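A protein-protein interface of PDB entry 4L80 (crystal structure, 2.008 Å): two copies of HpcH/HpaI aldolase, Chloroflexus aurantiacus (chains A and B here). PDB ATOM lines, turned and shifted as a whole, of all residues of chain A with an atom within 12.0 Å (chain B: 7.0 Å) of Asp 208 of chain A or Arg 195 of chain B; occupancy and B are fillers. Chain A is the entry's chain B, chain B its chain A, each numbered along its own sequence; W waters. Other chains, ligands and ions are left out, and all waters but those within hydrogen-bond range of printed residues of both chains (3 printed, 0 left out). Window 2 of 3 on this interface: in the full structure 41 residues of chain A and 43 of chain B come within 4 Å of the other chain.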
ATOM      1  N   GLY A 204      31.719  12.417  32.123  1.00  0.00           N
ATOM      2  CA  GLY A 204      30.331  12.031  31.971  1.00  0.00           C
ATOM      3  C   GLY A 204      29.520  12.971  31.106  1.00  0.00           C
ATOM      4  O   GLY A 204      29.976  14.057  30.750  1.00  0.00           O
ATOM      5  N   VAL A 205      28.311  12.546  30.763  1.00  0.00           N
ATOM      6  CA  VAL A 205      27.423  13.357  29.945  1.00  0.00           C
ATOM      7  C   VAL A 205      26.310  13.936  30.806  1.00  0.00           C
ATOM      8  O   VAL A 205      25.645  13.207  31.544  1.00  0.00           O
ATOM      9  CB  VAL A 205      26.809  12.535  28.795  1.00  0.00           C
ATOM     10  CG1 VAL A 205      25.809  13.373  28.007  1.00  0.00           C
ATOM     11  CG2 VAL A 205      27.905  12.005  27.884  1.00  0.00           C
ATOM     12  N   LEU A 206      26.117  15.247  30.716  1.00  0.00           N
ATOM     13  CA  LEU A 206      25.073  15.916  31.481  1.00  0.00           C
ATOM     14  C   LEU A 206      23.773  15.938  30.687  1.00  0.00           C
ATOM     15  O   LEU A 206      23.763  16.273  29.502  1.00  0.00           O
ATOM     16  CB  LEU A 206      25.498  17.340  31.844  1.00  0.00           C
ATOM     17  CG  LEU A 206      24.582  18.100  32.808  1.00  0.00           C
ATOM     18  CD1 LEU A 206      24.595  17.456  34.184  1.00  0.00           C
ATOM     19  CD2 LEU A 206      24.982  19.566  32.895  1.00  0.00           C
ATOM     20  N   ALA A 207      22.679  15.572  31.344  1.00  0.00           N
ATOM     21  CA  ALA A 207      21.376  15.547  30.696  1.00  0.00           C
ATOM     22  C   ALA A 207      20.882  16.961  30.416  1.00  0.00           C
ATOM     23  O   ALA A 207      21.362  17.925  31.013  1.00  0.00           O
ATOM     24  CB  ALA A 207      20.371  14.793  31.556  1.00  0.00           C
ATOM     25  N   ASP A 208      19.928  17.077  29.497  1.00  0.00           N
ATOM     26  CA  ASP A 208      19.284  18.353  29.206  1.00  0.00           C
ATOM     27  C   ASP A 208      18.554  18.846  30.453  1.00  0.00           C
ATOM     28  O   ASP A 208      18.223  18.044  31.323  1.00  0.00           O
ATOM     29  CB  ASP A 208      18.298  18.188  28.047  1.00  0.00           C
ATOM     30  CG  ASP A 208      18.990  18.093  26.699  1.00  0.00           C
ATOM     31  OD1 ASP A 208      20.230  17.958  26.668  1.00  0.00           O
ATOM     32  OD2 ASP A 208      18.291  18.151  25.667  1.00  0.00           O
ATOM     33  N   PRO A 209      18.322  20.169  30.557  1.00  0.00           N
ATOM     34  CA  PRO A 209      17.552  20.717  31.682  1.00  0.00           C
ATOM     35  C   PRO A 209      16.187  20.041  31.807  1.00  0.00           C
ATOM     36  O   PRO A 209      15.499  19.874  30.798  1.00  0.00           O
ATOM     37  CB  PRO A 209      17.390  22.189  31.303  1.00  0.00           C
ATOM     38  CG  PRO A 209      18.594  22.488  30.474  1.00  0.00           C
ATOM     39  CD  PRO A 209      18.860  21.231  29.688  1.00  0.00           C
ATOM     40  N   GLN A 210      15.813  19.654  33.024  1.00  0.00           N
ATOM     41  CA  GLN A 210      14.617  18.836  33.236  1.00  0.00           C
ATOM     42  C   GLN A 210      13.317  19.627  33.396  1.00  0.00           C
ATOM     43  O   GLN A 210      13.337  20.824  33.686  1.00  0.00           O
ATOM     44  CB  GLN A 210      14.812  17.880  34.416  1.00  0.00           C
ATOM     45  CG  GLN A 210      15.291  16.493  34.015  1.00  0.00           C
ATOM     46  CD  GLN A 210      16.614  16.527  33.279  1.00  0.00           C
ATOM     47  OE1 GLN A 210      17.655  16.823  33.865  1.00  0.00           O
ATOM     48  NE2 GLN A 210      16.579  16.237  31.981  1.00  0.00           N
ATOM     49  N   GLU A 211      12.201  18.915  33.226  1.00  0.00           N
ATOM     50  CA  GLU A 211      10.846  19.474  33.106  1.00  0.00           C
ATOM     51  C   GLU A 211      10.524  20.729  33.924  1.00  0.00           C
ATOM     52  O   GLU A 211       9.867  21.644  33.426  1.00  0.00           O
ATOM     53  CB  GLU A 211       9.801  18.390  33.402  1.00  0.00           C
ATOM     54  CG  GLU A 211       9.969  17.716  34.755  1.00  0.00           C
ATOM     55  CD  GLU A 211       8.810  16.803  35.104  1.00  0.00           C
ATOM     56  OE1 GLU A 211       7.655  17.151  34.780  1.00  0.00           O
ATOM     57  OE2 GLU A 211       9.056  15.733  35.701  1.00  0.00           O
ATOM     58  N   GLY A 212      10.976  20.766  35.172  1.00  0.00           N
ATOM     59  CA  GLY A 212      10.717  21.902  36.036  1.00  0.00           C
ATOM     60  C   GLY A 212      11.816  22.090  37.059  1.00  0.00           C
ATOM     61  O   GLY A 212      11.661  21.693  38.215  1.00  0.00           O
ATOM     62  N   GLN A 213      12.919  22.658  36.597  1.00  0.00           N
ATOM     63  CA  GLN A 213      14.047  22.925  37.438  1.00  0.00           C
ATOM     64  C   GLN A 213      14.829  21.677  37.834  1.00  0.00           C
ATOM     65  O   GLN A 213      15.978  21.777  38.165  1.00  0.00           O
ATOM     66  CB  GLN A 213      13.555  23.662  38.674  1.00  0.00           C
ATOM     67  CG  GLN A 213      13.545  22.873  39.966  1.00  0.00           C
ATOM     68  CD  GLN A 213      14.623  23.294  40.961  1.00  0.00           C
ATOM     69  OE1 GLN A 213      15.540  24.052  40.642  1.00  0.00           O
ATOM     70  NE2 GLN A 213      14.496  22.815  42.190  1.00  0.00           N
ATOM     71  N   ALA A 214      14.167  20.524  37.818  1.00  0.00           N
ATOM     72  CA  ALA A 214      14.641  19.248  38.366  1.00  0.00           C
ATOM     73  C   ALA A 214      16.109  18.934  38.084  1.00  0.00           C
ATOM     74  O   ALA A 214      16.641  19.296  37.033  1.00  0.00           O
ATOM     75  CB  ALA A 214      13.753  18.103  37.886  1.00  0.00           C
ATOM     76  N   GLU A 215      16.746  18.254  39.033  1.00  0.00           N
ATOM     77  CA  GLU A 215      18.173  17.948  38.965  1.00  0.00           C
ATOM     78  C   GLU A 215      18.542  17.160  37.708  1.00  0.00           C
ATOM     79  O   GLU A 215      17.763  16.337  37.225  1.00  0.00           O
ATOM     80  CB  GLU A 215      18.620  17.203  40.227  1.00  0.00           C
ATOM     81  CG  GLU A 215      20.124  17.014  40.340  1.00  0.00           C
ATOM     82  CD  GLU A 215      20.576  16.760  41.766  1.00  0.00           C
ATOM     83  OE1 GLU A 215      19.735  16.859  42.685  1.00  0.00           O
ATOM     84  OE2 GLU A 215      21.774  16.467  41.968  1.00  0.00           O
ATOM     85  N   ARG A 216      19.734  17.424  37.182  1.00  0.00           N
ATOM     86  CA  ARG A 216      20.160  16.842  35.918  1.00  0.00           C
ATOM     87  C   ARG A 216      21.049  15.624  36.123  1.00  0.00           C
ATOM     88  O   ARG A 216      22.097  15.715  36.762  1.00  0.00           O
ATOM     89  CB  ARG A 216      20.873  17.898  35.070  1.00  0.00           C
ATOM     90  CG  ARG A 216      19.986  19.087  34.735  1.00  0.00           C
ATOM     91  CD  ARG A 216      20.784  20.278  34.231  1.00  0.00           C
ATOM     92  NE  ARG A 216      21.294  20.079  32.879  1.00  0.00           N
ATOM     93  CZ  ARG A 216      21.870  21.034  32.155  1.00  0.00           C
ATOM     94  NH1 ARG A 216      22.005  22.254  32.656  1.00  0.00           N
ATOM     95  NH2 ARG A 216      22.308  20.772  30.931  1.00  0.00           N
ATOM     96  N   PRO A 217      20.613  14.469  35.595  1.00  0.00           N
ATOM     97  CA  PRO A 217      21.380  13.221  35.643  1.00  0.00           C
ATOM     98  C   PRO A 217      22.738  13.358  34.958  1.00  0.00           C
ATOM     99  O   PRO A 217      22.854  14.017  33.922  1.00  0.00           O
ATOM    100  CB  PRO A 217      20.499  12.240  34.864  1.00  0.00           C
ATOM    101  CG  PRO A 217      19.121  12.779  35.008  1.00  0.00           C
ATOM    102  CD  PRO A 217      19.281  14.272  34.998  1.00  0.00           C
ATOM    103  N   PHE A 218      23.752  12.733  35.546  1.00  0.00           N
ATOM    104  CA  PHE A 218      25.105  12.768  35.013  1.00  0.00           C
ATOM    105  C   PHE A 218      25.580  11.337  34.788  1.00  0.00           C
ATOM    106  O   PHE A 218      25.786  10.590  35.742  1.00  0.00           O
ATOM    107  CB  PHE A 218      26.023  13.493  35.997  1.00  0.00           C
ATOM    108  CG  PHE A 218      27.418  13.715  35.488  1.00  0.00           C
ATOM    109  CD1 PHE A 218      27.665  14.642  34.490  1.00  0.00           C
ATOM    110  CD2 PHE A 218      28.484  13.018  36.028  1.00  0.00           C
ATOM    111  CE1 PHE A 218      28.945  14.855  34.027  1.00  0.00           C
ATOM    112  CE2 PHE A 218      29.769  13.230  35.571  1.00  0.00           C
ATOM    113  CZ  PHE A 218      29.999  14.155  34.571  1.00  0.00           C
ATOM    114  N   TYR A 219      25.739  10.954  33.525  1.00  0.00           N
ATOM    115  CA  TYR A 219      26.075   9.576  33.175  1.00  0.00           C
ATOM    116  C   TYR A 219      27.568   9.414  32.910  1.00  0.00           C
ATOM    117  O   TYR A 219      28.079   9.928  31.916  1.00  0.00           O
ATOM    118  CB  TYR A 219      25.301   9.138  31.928  1.00  0.00           C
ATOM    119  CG  TYR A 219      23.809   9.372  31.987  1.00  0.00           C
ATOM    120  CD1 TYR A 219      22.949   8.386  32.457  1.00  0.00           C
ATOM    121  CD2 TYR A 219      23.257  10.573  31.560  1.00  0.00           C
ATOM    122  CE1 TYR A 219      21.582   8.596  32.509  1.00  0.00           C
ATOM    123  CE2 TYR A 219      21.893  10.792  31.609  1.00  0.00           C
ATOM    124  CZ  TYR A 219      21.060   9.802  32.083  1.00  0.00           C
ATOM    125  OH  TYR A 219      19.704  10.020  32.130  1.00  0.00           O
ATOM    126  N   GLN A 221      31.107   8.004  31.698  1.00  0.00           N
ATOM    127  CA  GLN A 221      31.504   7.380  30.442  1.00  0.00           C
ATOM    128  C   GLN A 221      32.812   6.623  30.625  1.00  0.00           C
ATOM    129  O   GLN A 221      33.565   6.892  31.559  1.00  0.00           O
ATOM    130  CB  GLN A 221      31.667   8.445  29.355  1.00  0.00           C
ATOM    131  CG  GLN A 221      30.455   9.346  29.188  1.00  0.00           C
ATOM    132  CD  GLN A 221      29.279   8.631  28.552  1.00  0.00           C
ATOM    133  OE1 GLN A 221      29.404   8.044  27.476  1.00  0.00           O
ATOM    134  NE2 GLN A 221      28.127   8.678  29.214  1.00  0.00           N
ATOM    135  N   PRO B 182      32.807  21.083  16.487  1.00  0.00           N
ATOM    136  CA  PRO B 182      31.656  20.175  16.575  1.00  0.00           C
ATOM    137  C   PRO B 182      30.530  20.513  15.603  1.00  0.00           C
ATOM    138  O   PRO B 182      29.841  19.604  15.140  1.00  0.00           O
ATOM    139  CB  PRO B 182      31.166  20.367  18.018  1.00  0.00           C
ATOM    140  CG  PRO B 182      32.313  20.961  18.749  1.00  0.00           C
ATOM    141  CD  PRO B 182      33.012  21.817  17.746  1.00  0.00           C
ATOM    142  N   ALA B 183      30.342  21.795  15.308  1.00  0.00           N
ATOM    143  CA  ALA B 183      29.240  22.221  14.451  1.00  0.00           C
ATOM    144  C   ALA B 183      29.463  21.808  13.000  1.00  0.00           C
ATOM    145  O   ALA B 183      28.652  21.081  12.426  1.00  0.00           O
ATOM    146  CB  ALA B 183      29.025  23.727  14.561  1.00  0.00           C
ATOM    147  N   ALA B 186      29.760  17.919  12.660  1.00  0.00           N
ATOM    148  CA  ALA B 186      28.453  17.274  12.633  1.00  0.00           C
ATOM    149  C   ALA B 186      27.805  17.421  11.256  1.00  0.00           C
ATOM    150  O   ALA B 186      27.261  16.460  10.712  1.00  0.00           O
ATOM    151  CB  ALA B 186      27.548  17.839  13.722  1.00  0.00           C
ATOM    152  N   LYS B 192      23.040  13.896  12.993  1.00  0.00           N
ATOM    153  CA  LYS B 192      21.708  14.488  12.922  1.00  0.00           C
ATOM    154  C   LYS B 192      21.350  15.305  14.159  1.00  0.00           C
ATOM    155  O   LYS B 192      20.539  14.886  14.986  1.00  0.00           O
ATOM    156  CB  LYS B 192      20.656  13.412  12.642  1.00  0.00           C
ATOM    157  CG  LYS B 192      20.834  12.742  11.287  1.00  0.00           C
ATOM    158  CD  LYS B 192      20.743  13.758  10.159  1.00  0.00           C
ATOM    159  CE  LYS B 192      20.835  13.094   8.790  1.00  0.00           C
ATOM    160  NZ  LYS B 192      22.148  12.418   8.574  1.00  0.00           N
ATOM    161  N   THR B 193      21.971  16.476  14.266  1.00  0.00           N
ATOM    162  CA  THR B 193      21.700  17.418  15.344  1.00  0.00           C
ATOM    163  C   THR B 193      22.136  18.816  14.922  1.00  0.00           C
ATOM    164  O   THR B 193      22.972  18.972  14.030  1.00  0.00           O
ATOM    165  CB  THR B 193      22.431  17.032  16.649  1.00  0.00           C
ATOM    166  OG1 THR B 193      22.203  18.042  17.642  1.00  0.00           O
ATOM    167  CG2 THR B 193      23.928  16.898  16.408  1.00  0.00           C
ATOM    168  N   THR B 194      21.557  19.830  15.560  1.00  0.00           N
ATOM    169  CA  THR B 194      21.941  21.212  15.300  1.00  0.00           C
ATOM    170  C   THR B 194      22.693  21.779  16.493  1.00  0.00           C
ATOM    171  O   THR B 194      23.092  22.944  16.493  1.00  0.00           O
ATOM    172  CB  THR B 194      20.719  22.101  15.015  1.00  0.00           C
ATOM    173  OG1 THR B 194      19.750  21.927  16.054  1.00  0.00           O
ATOM    174  CG2 THR B 194      20.097  21.742  13.674  1.00  0.00           C
ATOM    175  N   ARG B 195      22.881  20.947  17.512  1.00  0.00           N
ATOM    176  CA  ARG B 195      23.601  21.362  18.710  1.00  0.00           C
ATOM    177  C   ARG B 195      25.091  21.504  18.425  1.00  0.00           C
ATOM    178  O   ARG B 195      25.611  20.920  17.472  1.00  0.00           O
ATOM    179  CB  ARG B 195      23.375  20.369  19.852  1.00  0.00           C
ATOM    180  CG  ARG B 195      21.923  20.234  20.269  1.00  0.00           C
ATOM    181  CD  ARG B 195      21.773  19.313  21.464  1.00  0.00           C
ATOM    182  NE  ARG B 195      20.377  19.173  21.870  1.00  0.00           N
ATOM    183  CZ  ARG B 195      19.988  18.690  23.044  1.00  0.00           C
ATOM    184  NH1 ARG B 195      20.890  18.304  23.936  1.00  0.00           N
ATOM    185  NH2 ARG B 195      18.697  18.599  23.332  1.00  0.00           N
ATOM    186  N   VAL B 196      25.767  22.290  19.254  1.00  0.00           N
ATOM    187  CA  VAL B 196      27.197  22.518  19.112  1.00  0.00           C
ATOM    188  C   VAL B 196      27.916  22.009  20.355  1.00  0.00           C
ATOM    189  O   VAL B 196      28.086  22.740  21.329  1.00  0.00           O
ATOM    190  CB  VAL B 196      27.503  24.014  18.897  1.00  0.00           C
ATOM    191  CG1 VAL B 196      28.999  24.234  18.687  1.00  0.00           C
ATOM    192  CG2 VAL B 196      26.712  24.542  17.713  1.00  0.00           C
ATOM    193  N   GLY B 197      28.321  20.744  20.321  1.00  0.00           N
ATOM    194  CA  GLY B 197      28.918  20.105  21.479  1.00  0.00           C
ATOM    195  C   GLY B 197      27.865  19.661  22.478  1.00  0.00           C
ATOM    196  O   GLY B 197      26.666  19.830  22.247  1.00  0.00           O
ATOM    197  N   GLY B 198      28.312  19.088  23.592  1.00  0.00           N
ATOM    198  CA  GLY B 198      27.406  18.630  24.628  1.00  0.00           C
ATOM    199  C   GLY B 198      26.714  17.327  24.268  1.00  0.00           C
ATOM    200  O   GLY B 198      26.915  16.785  23.182  1.00  0.00           O
ATOM    201  N   GLY B 199      25.892  16.826  25.184  1.00  0.00           N
ATOM    202  CA  GLY B 199      25.206  15.566  24.972  1.00  0.00           C
ATOM    203  C   GLY B 199      24.004  15.676  24.055  1.00  0.00           C
ATOM    204  O   GLY B 199      23.643  16.764  23.605  1.00  0.00           O
ATOM    205  N   HIS B 200      23.395  14.534  23.764  1.00  0.00           N
ATOM    206  CA  HIS B 200      22.127  14.492  23.053  1.00  0.00           C
ATOM    207  C   HIS B 200      21.272  13.397  23.682  1.00  0.00           C
ATOM    208  O   HIS B 200      21.726  12.263  23.841  1.00  0.00           O
ATOM    209  CB  HIS B 200      22.335  14.222  21.563  1.00  0.00           C
ATOM    210  CG  HIS B 200      21.130  14.519  20.724  1.00  0.00           C
ATOM    211  ND1 HIS B 200      19.978  13.765  20.781  1.00  0.00           N
ATOM    212  CD2 HIS B 200      20.897  15.490  19.810  1.00  0.00           C
ATOM    213  CE1 HIS B 200      19.088  14.258  19.939  1.00  0.00           C
ATOM    214  NE2 HIS B 200      19.621  15.305  19.335  1.00  0.00           N
ATOM    215  N   PRO B 201      20.031  13.738  24.056  1.00  0.00           N
ATOM    216  CA  PRO B 201      19.141  12.806  24.759  1.00  0.00           C
ATOM    217  C   PRO B 201      18.804  11.551  23.954  1.00  0.00           C
ATOM    218  O   PRO B 201      18.371  10.559  24.537  1.00  0.00           O
ATOM    219  CB  PRO B 201      17.876  13.644  25.002  1.00  0.00           C
ATOM    220  CG  PRO B 201      17.945  14.755  23.998  1.00  0.00           C
ATOM    221  CD  PRO B 201      19.404  15.055  23.849  1.00  0.00           C
ATOM    222  N   GLN B 220      22.598   7.840  28.677  1.00  0.00           N
ATOM    223  CA  GLN B 220      23.132   8.716  27.635  1.00  0.00           C
ATOM    224  C   GLN B 220      24.618   8.469  27.393  1.00  0.00           C
ATOM    225  O   GLN B 220      25.373   8.176  28.325  1.00  0.00           O
ATOM    226  CB  GLN B 220      22.895  10.192  27.969  1.00  0.00           C
ATOM    227  CG  GLN B 220      21.464  10.654  27.768  1.00  0.00           C
ATOM    228  CD  GLN B 220      21.305  12.152  27.944  1.00  0.00           C
ATOM    229  OE1 GLN B 220      20.341  12.617  28.546  1.00  0.00           O
ATOM    230  NE2 GLN B 220      22.253  12.917  27.410  1.00  0.00           N
ATOM    231  N   LEU B 223      28.740  11.641  22.487  1.00  0.00           N
ATOM    232  CA  LEU B 223      28.839  11.695  21.029  1.00  0.00           C
ATOM    233  C   LEU B 223      30.275  11.869  20.554  1.00  0.00           C
ATOM    234  O   LEU B 223      30.620  11.464  19.446  1.00  0.00           O
ATOM    235  CB  LEU B 223      28.009  12.859  20.481  1.00  0.00           C
ATOM    236  CG  LEU B 223      26.489  12.725  20.406  1.00  0.00           C
ATOM    237  CD1 LEU B 223      25.876  14.086  20.160  1.00  0.00           C
ATOM    238  CD2 LEU B 223      26.098  11.758  19.297  1.00  0.00           C
ATOM    239  N   TRP B 224      31.109  12.467  21.401  1.00  0.00           N
ATOM    240  CA  TRP B 224      32.401  12.984  20.963  1.00  0.00           C
ATOM    241  C   TRP B 224      33.605  12.198  21.470  1.00  0.00           C
ATOM    242  O   TRP B 224      34.744  12.623  21.281  1.00  0.00           O
ATOM    243  CB  TRP B 224      32.520  14.460  21.361  1.00  0.00           C
ATOM    244  CG  TRP B 224      31.377  15.268  20.839  1.00  0.00           C
ATOM    245  CD1 TRP B 224      30.321  15.759  21.553  1.00  0.00           C
ATOM    246  CD2 TRP B 224      31.154  15.647  19.477  1.00  0.00           C
ATOM    247  NE1 TRP B 224      29.460  16.432  20.717  1.00  0.00           N
ATOM    248  CE2 TRP B 224      29.949  16.376  19.438  1.00  0.00           C
ATOM    249  CE3 TRP B 224      31.860  15.444  18.286  1.00  0.00           C
ATOM    250  CZ2 TRP B 224      29.436  16.905  18.256  1.00  0.00           C
ATOM    251  CZ3 TRP B 224      31.348  15.970  17.114  1.00  0.00           C
ATOM    252  CH2 TRP B 224      30.148  16.691  17.107  1.00  0.00           C
ATOM    253  N   GLY B 248      28.250  25.789  21.970  1.00  0.00           N
ATOM    254  CA  GLY B 248      27.283  26.727  21.427  1.00  0.00           C
ATOM    255  C   GLY B 248      26.214  27.245  22.371  1.00  0.00           C
ATOM    256  O   GLY B 248      25.692  28.341  22.171  1.00  0.00           O
ATOM    257  N   ASP B 252      23.807  27.735  28.979  1.00  0.00           N
ATOM    258  CA  ASP B 252      23.897  26.512  29.771  1.00  0.00           C
ATOM    259  C   ASP B 252      25.321  26.308  30.279  1.00  0.00           C
ATOM    260  O   ASP B 252      26.079  25.510  29.728  1.00  0.00           O
ATOM    261  CB  ASP B 252      23.443  25.306  28.944  1.00  0.00           C
ATOM    262  CG  ASP B 252      23.100  24.098  29.801  1.00  0.00           C
ATOM    263  OD1 ASP B 252      23.570  24.022  30.957  1.00  0.00           O
ATOM    264  OD2 ASP B 252      22.358  23.215  29.314  1.00  0.00           O
ATOM    265  N   ALA B 255      26.248  22.569  31.454  1.00  0.00           N
ATOM    266  CA  ALA B 255      26.573  21.657  30.360  1.00  0.00           C
ATOM    267  C   ALA B 255      27.899  22.045  29.720  1.00  0.00           C
ATOM    268  O   ALA B 255      28.656  21.182  29.274  1.00  0.00           O
ATOM    269  CB  ALA B 255      25.464  21.638  29.323  1.00  0.00           C
HETATM  270  O   HOH W   1      22.256  15.831  27.217  1.00  0.00           O
HETATM  271  O   HOH W   2      25.068  18.384  27.730  1.00  0.00           O
HETATM  272  O   HOH W   3      18.893  14.842  28.313  1.00  0.00           O
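The guanidinium group (NH2) of Arg 195 of chain B lies within salt-bridge range of the side-chain carboxylate (OD2) of Asp 208 of chain A.
The backbone carbonyl oxygen of Gln 220 of chain B lies within hydrogen-bond range of the side-chain amide nitrogen of Gln 221 of chain A, at 2.9 Å.
NH1 of Arg 216 of chain A is in salt-bridge range of OD1 of Asp 252 of chain B (2.9 Å).
The side-chain hydroxyl of Thr 193 of chain B lies within hydrogen-bond range of the backbone NH of Arg 195 of chain B (3.0 Å).
OD1 of Asp 252 of chain B sits at hydrogen-bond distance from N of Ala 255 of chain B (3.1 Å).
The backbone NH of Val 205 of chain A sits at hydrogen-bond distance from the backbone carbonyl oxygen of Tyr 219 of chain A (2.9 Å).
O of Pro 217 of chain A is in hydrogen-bond range of N of Ala 207 of chain A, 3.0 Å away.
O of Asp 208 of chain A is in hydrogen-bond range of NE2 of Gln 210 of chain A.
O of Tyr 219 of chain A is in hydrogen-bond range of NE2 of Gln 221 of chain A, at 3.0 Å.
Val 205 of chain A touches Gly 199 of chain B (CG1 to CA, 3.8 Å).
Gln 220 of chain B touches Val 205 of chain A.
Leu 206 of chain A touches Ala 255 of chain B.
Ala 207 of chain A touches Gln 220 of chain B (CB to OE1, 3.7 Å).
CD of Pro 201 of chain B touches OD2 of Asp 208 of chain A (3.8 Å).
Arg 216 of chain A touches Ala 255 of chain B.
CD2 of Tyr 219 of chain A touches CB of Gln 220 of chain B, 3.6 Å away.
Of the printed residues of chain B, Ala 207 of chain A touches Gln 220 (3.7 Å).
Asp 208 of chain A touches just these residues of chain B: Arg 195 and Pro 201.
Pro 209 of chain A touches none of the printed residues of chain B.
Of the printed residues of chain B, Arg 216 of chain A touches Asp 252 and Ala 255.
Of the printed residues of chain B, Tyr 219 of chain A touches Gln 220.
No residue of chain A comes within 4 Å of Pro 182 of chain B.
No residue of chain A comes within 4 Å of Ala 183 of chain B.
Lys 192 of chain B touches none of the printed residues of chain A.
No residue of chain A comes within 4 Å of Thr 194 of chain B.
Arg 195 of chain B touches just one residue of chain A: Asp 208.
No residue of chain A comes within 4 Å of Val 196 of chain B.
Of chain A, only Val 205 comes within 4 Å of Gly 199 of chain B.
No residue of chain A comes within 4 Å of His 200 of chain B.
Of the printed residues of chain A, Gln 220 of chain B touches Val 205, Ala 207, Tyr 219 and Gln 221.
Gly 248 of chain B touches none of the printed residues of chain A.
Of the printed residues of chain A, Ala 255 of chain B touches Leu 206 (3.6 Å) and Arg 216 (3.6 Å).
The nearest residue of chain B that does not touch Asp 208 of chain A is Gln 220 of chain B (4.6 Å).
The nearest residue of chain A that does not touch Arg 195 of chain B is Leu 206 of chain A (6.6 Å).
Along chain A the printed residues that touch a printed residue of chain B span positions 205 to 221.
Among the printed residues, 10 pairs touch across the chains.
No position is printed for both chains.
Of the 10 pairs that touch across the chains among the printed residues, none has its exchanged pair printed and touching as well.
Water W3 lies within hydrogen-bond range of the side-chain amide oxygen of Gln 220 of chain B (2.7 Å) and the backbone NH of Asp 208 of chain A (2.7 Å).
Water W1 lies within hydrogen-bond range of the backbone carbonyl oxygen of Leu 206 of chain A (2.8 Å), the side-chain amide nitrogen of Gln 220 of chain B (2.9 Å) and the side-chain carboxylate of Asp 208 of chain A (3.0 Å).
Water W2 bridges the backbone carbonyl oxygen of Leu 206 of chain A and the backbone NH of Gly 199 of chain B.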
